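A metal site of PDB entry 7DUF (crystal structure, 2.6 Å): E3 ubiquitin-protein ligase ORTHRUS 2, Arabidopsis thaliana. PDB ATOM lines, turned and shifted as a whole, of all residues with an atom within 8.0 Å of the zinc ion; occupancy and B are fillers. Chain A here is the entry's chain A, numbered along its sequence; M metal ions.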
ATOM      1  N   THR A  33      23.385 -31.264  17.517  1.00  0.00           N
ATOM      2  CA  THR A  33      23.683 -29.935  18.029  1.00  0.00           C
ATOM      3  C   THR A  33      24.338 -29.108  16.926  1.00  0.00           C
ATOM      4  O   THR A  33      25.113 -29.623  16.124  1.00  0.00           O
ATOM      5  CB  THR A  33      24.602 -29.998  19.253  1.00  0.00           C
ATOM      6  OG1 THR A  33      25.974 -29.979  18.838  1.00  0.00           O
ATOM      7  CG2 THR A  33      24.330 -31.249  20.066  1.00  0.00           C
ATOM      8  N   CYS A  34      24.005 -27.818  16.897  1.00  0.00           N
ATOM      9  CA  CYS A  34      24.525 -26.926  15.879  1.00  0.00           C
ATOM     10  C   CYS A  34      26.006 -26.653  16.105  1.00  0.00           C
ATOM     11  O   CYS A  34      26.487 -26.595  17.237  1.00  0.00           O
ATOM     12  CB  CYS A  34      23.739 -25.611  15.878  1.00  0.00           C
ATOM     13  SG  CYS A  34      24.256 -24.403  14.639  1.00  0.00           S
ATOM     14  N   GLY A  35      26.747 -26.501  15.001  1.00  0.00           N
ATOM     15  CA  GLY A  35      28.148 -26.149  15.098  1.00  0.00           C
ATOM     16  C   GLY A  35      28.416 -24.686  15.326  1.00  0.00           C
ATOM     17  O   GLY A  35      29.576 -24.301  15.537  1.00  0.00           O
ATOM     18  N   THR A  36      27.381 -23.848  15.299  1.00  0.00           N
ATOM     19  CA  THR A  36      27.527 -22.409  15.490  1.00  0.00           C
ATOM     20  C   THR A  36      26.980 -21.985  16.844  1.00  0.00           C
ATOM     21  O   THR A  36      27.744 -21.520  17.694  1.00  0.00           O
ATOM     22  CB  THR A  36      26.823 -21.662  14.347  1.00  0.00           C
ATOM     23  OG1 THR A  36      27.550 -21.861  13.125  1.00  0.00           O
ATOM     24  CG2 THR A  36      26.760 -20.162  14.648  1.00  0.00           C
ATOM     25  N   CYS A  37      25.676 -22.125  17.072  1.00  0.00           N
ATOM     26  CA  CYS A  37      25.062 -21.733  18.342  1.00  0.00           C
ATOM     27  C   CYS A  37      25.044 -22.861  19.367  1.00  0.00           C
ATOM     28  O   CYS A  37      24.729 -22.597  20.539  1.00  0.00           O
ATOM     29  CB  CYS A  37      23.628 -21.248  18.091  1.00  0.00           C
ATOM     30  SG  CYS A  37      22.518 -22.525  17.467  1.00  0.00           S
ATOM     31  N   VAL A  38      25.380 -24.083  18.960  1.00  0.00           N
ATOM     32  CA  VAL A  38      25.366 -25.270  19.822  1.00  0.00           C
ATOM     33  C   VAL A  38      23.990 -25.405  20.470  1.00  0.00           C
ATOM     34  O   VAL A  38      23.875 -25.460  21.700  1.00  0.00           O
ATOM     35  CB  VAL A  38      26.492 -25.220  20.865  1.00  0.00           C
ATOM     36  CG1 VAL A  38      26.714 -26.613  21.452  1.00  0.00           C
ATOM     37  CG2 VAL A  38      27.779 -24.703  20.240  1.00  0.00           C
ATOM     38  N   THR A  39      22.952 -25.432  19.658  1.00  0.00           N
ATOM     39  CA  THR A  39      21.620 -25.736  20.154  1.00  0.00           C
ATOM     40  C   THR A  39      21.239 -27.148  19.747  1.00  0.00           C
ATOM     41  O   THR A  39      21.406 -27.513  18.571  1.00  0.00           O
ATOM     42  CB  THR A  39      20.592 -24.750  19.598  1.00  0.00           C
ATOM     43  OG1 THR A  39      21.076 -23.409  19.755  1.00  0.00           O
ATOM     44  CG2 THR A  39      19.260 -24.892  20.331  1.00  0.00           C
ATOM     45  N   PRO A  40      20.755 -27.980  20.669  1.00  0.00           N
ATOM     46  CA  PRO A  40      20.340 -29.331  20.281  1.00  0.00           C
ATOM     47  C   PRO A  40      19.004 -29.314  19.558  1.00  0.00           C
ATOM     48  O   PRO A  40      18.071 -28.591  19.938  1.00  0.00           O
ATOM     49  CB  PRO A  40      20.244 -30.066  21.619  1.00  0.00           C
ATOM     50  CG  PRO A  40      19.940 -28.997  22.610  1.00  0.00           C
ATOM     51  CD  PRO A  40      20.633 -27.742  22.114  1.00  0.00           C
ATOM     52  N   TRP A  41      18.915 -30.107  18.499  1.00  0.00           N
ATOM     53  CA  TRP A  41      17.696 -30.231  17.712  1.00  0.00           C
ATOM     54  C   TRP A  41      17.325 -31.699  17.584  1.00  0.00           C
ATOM     55  O   TRP A  41      18.204 -32.564  17.488  1.00  0.00           O
ATOM     56  CB  TRP A  41      17.872 -29.632  16.310  1.00  0.00           C
ATOM     57  CG  TRP A  41      18.014 -28.139  16.305  1.00  0.00           C
ATOM     58  CD1 TRP A  41      19.087 -27.419  16.743  1.00  0.00           C
ATOM     59  CD2 TRP A  41      17.056 -27.186  15.835  1.00  0.00           C
ATOM     60  NE1 TRP A  41      18.854 -26.081  16.577  1.00  0.00           N
ATOM     61  CE2 TRP A  41      17.610 -25.901  16.018  1.00  0.00           C
ATOM     62  CE3 TRP A  41      15.780 -27.282  15.278  1.00  0.00           C
ATOM     63  CZ2 TRP A  41      16.942 -24.735  15.665  1.00  0.00           C
ATOM     64  CZ3 TRP A  41      15.105 -26.123  14.929  1.00  0.00           C
ATOM     65  CH2 TRP A  41      15.694 -24.867  15.118  1.00  0.00           C
ATOM     66  N   TRP A  59      27.176 -29.826  10.947  1.00  0.00           N
ATOM     67  CA  TRP A  59      25.773 -29.481  10.771  1.00  0.00           C
ATOM     68  C   TRP A  59      25.480 -28.099  11.333  1.00  0.00           C
ATOM     69  O   TRP A  59      25.979 -27.729  12.401  1.00  0.00           O
ATOM     70  CB  TRP A  59      24.872 -30.514  11.440  1.00  0.00           C
ATOM     71  CG  TRP A  59      23.410 -30.234  11.239  1.00  0.00           C
ATOM     72  CD1 TRP A  59      22.713 -30.360  10.071  1.00  0.00           C
ATOM     73  CD2 TRP A  59      22.482 -29.766  12.217  1.00  0.00           C
ATOM     74  NE1 TRP A  59      21.399 -30.000  10.267  1.00  0.00           N
ATOM     75  CE2 TRP A  59      21.233 -29.631  11.575  1.00  0.00           C
ATOM     76  CE3 TRP A  59      22.578 -29.444  13.577  1.00  0.00           C
ATOM     77  CZ2 TRP A  59      20.089 -29.197  12.247  1.00  0.00           C
ATOM     78  CZ3 TRP A  59      21.450 -29.013  14.242  1.00  0.00           C
ATOM     79  CH2 TRP A  59      20.221 -28.896  13.580  1.00  0.00           C
ATOM     80  N   HIS A  60      24.660 -27.347  10.613  1.00  0.00           N
ATOM     81  CA  HIS A  60      24.253 -26.007  11.021  1.00  0.00           C
ATOM     82  C   HIS A  60      22.729 -25.948  11.089  1.00  0.00           C
ATOM     83  O   HIS A  60      22.047 -26.318  10.124  1.00  0.00           O
ATOM     84  CB  HIS A  60      24.797 -24.952  10.057  1.00  0.00           C
ATOM     85  CG  HIS A  60      26.298 -24.872  10.051  1.00  0.00           C
ATOM     86  ND1 HIS A  60      27.052 -25.024  11.190  1.00  0.00           N
ATOM     87  CD2 HIS A  60      27.181 -24.670   9.033  1.00  0.00           C
ATOM     88  CE1 HIS A  60      28.335 -24.924  10.885  1.00  0.00           C
ATOM     89  NE2 HIS A  60      28.435 -24.697   9.583  1.00  0.00           N
ATOM     90  N   CYS A  61      22.214 -25.501  12.229  1.00  0.00           N
ATOM     91  CA  CYS A  61      20.793 -25.584  12.513  1.00  0.00           C
ATOM     92  C   CYS A  61      20.002 -24.636  11.604  1.00  0.00           C
ATOM     93  O   CYS A  61      20.562 -23.693  11.036  1.00  0.00           O
ATOM     94  CB  CYS A  61      20.539 -25.258  13.984  1.00  0.00           C
ATOM     95  SG  CYS A  61      20.510 -23.511  14.390  1.00  0.00           S
ATOM     96  N   PRO A  62      18.706 -24.884  11.443  1.00  0.00           N
ATOM     97  CA  PRO A  62      17.894 -24.033  10.545  1.00  0.00           C
ATOM     98  C   PRO A  62      17.929 -22.551  10.901  1.00  0.00           C
ATOM     99  O   PRO A  62      17.790 -21.710  10.004  1.00  0.00           O
ATOM    100  CB  PRO A  62      16.485 -24.611  10.695  1.00  0.00           C
ATOM    101  CG  PRO A  62      16.709 -26.041  11.046  1.00  0.00           C
ATOM    102  CD  PRO A  62      17.925 -26.042  11.927  1.00  0.00           C
ATOM    103  N   ASP A  63      18.109 -22.207  12.182  1.00  0.00           N
ATOM    104  CA  ASP A  63      18.163 -20.798  12.551  1.00  0.00           C
ATOM    105  C   ASP A  63      19.496 -20.168  12.135  1.00  0.00           C
ATOM    106  O   ASP A  63      19.555 -18.953  11.920  1.00  0.00           O
ATOM    107  CB  ASP A  63      17.941 -20.640  14.054  1.00  0.00           C
ATOM    108  CG  ASP A  63      16.479 -20.480  14.412  1.00  0.00           C
ATOM    109  OD1 ASP A  63      15.757 -19.779  13.667  1.00  0.00           O
ATOM    110  OD2 ASP A  63      16.048 -21.046  15.427  1.00  0.00           O
ATOM    111  N   CYS A  64      20.552 -20.971  12.029  1.00  0.00           N
ATOM    112  CA  CYS A  64      21.860 -20.460  11.630  1.00  0.00           C
ATOM    113  C   CYS A  64      22.124 -20.575  10.140  1.00  0.00           C
ATOM    114  O   CYS A  64      22.965 -19.830   9.611  1.00  0.00           O
ATOM    115  CB  CYS A  64      22.968 -21.197  12.395  1.00  0.00           C
ATOM    116  SG  CYS A  64      23.061 -20.795  14.155  1.00  0.00           S
ATOM    117  N   SER A  65      21.447 -21.478   9.448  1.00  0.00           N
ATOM    118  CA  SER A  65      21.661 -21.676   8.018  1.00  0.00           C
ATOM    119  C   SER A  65      21.149 -20.484   7.210  1.00  0.00           C
ATOM    120  O   SER A  65      19.970 -20.149   7.260  1.00  0.00           O
ATOM    121  CB  SER A  65      20.976 -22.962   7.548  1.00  0.00           C
HETATM  122 ZN    ZN M   1      22.609 -22.841  15.166  1.00  0.00          ZN
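The backbone NH (N) of Cys 34 is in hydrogen-bond range of the backbone carbonyl oxygen (O) of Thr 39 (3.1 Å).
The side-chain sulfur of Cys 37 sits close to the side-chain hydroxyl of Thr 39 (2.8 Å).
SG of Cys 61 sits close to NE1 of Trp 41 (3.8 Å).
SG of Cys 34 sits close to N of Thr 36.
SG of Cys 61 lies close to N of Asp 63.
Four residues have an atom within 4 Å of the zinc ion: Cys 34, Cys 37, Cys 61 and Cys 64.
The zinc ion is bound by the side-chain sulfur (SG) of Cys 37, 2.3 Å away.
SG of Cys 64 is bound to the zinc ion.
The side-chain sulfur (SG) of Cys 34 is bound to the zinc ion.
The side-chain sulfur (SG) of Cys 61 binds the zinc ion (2.3 Å).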
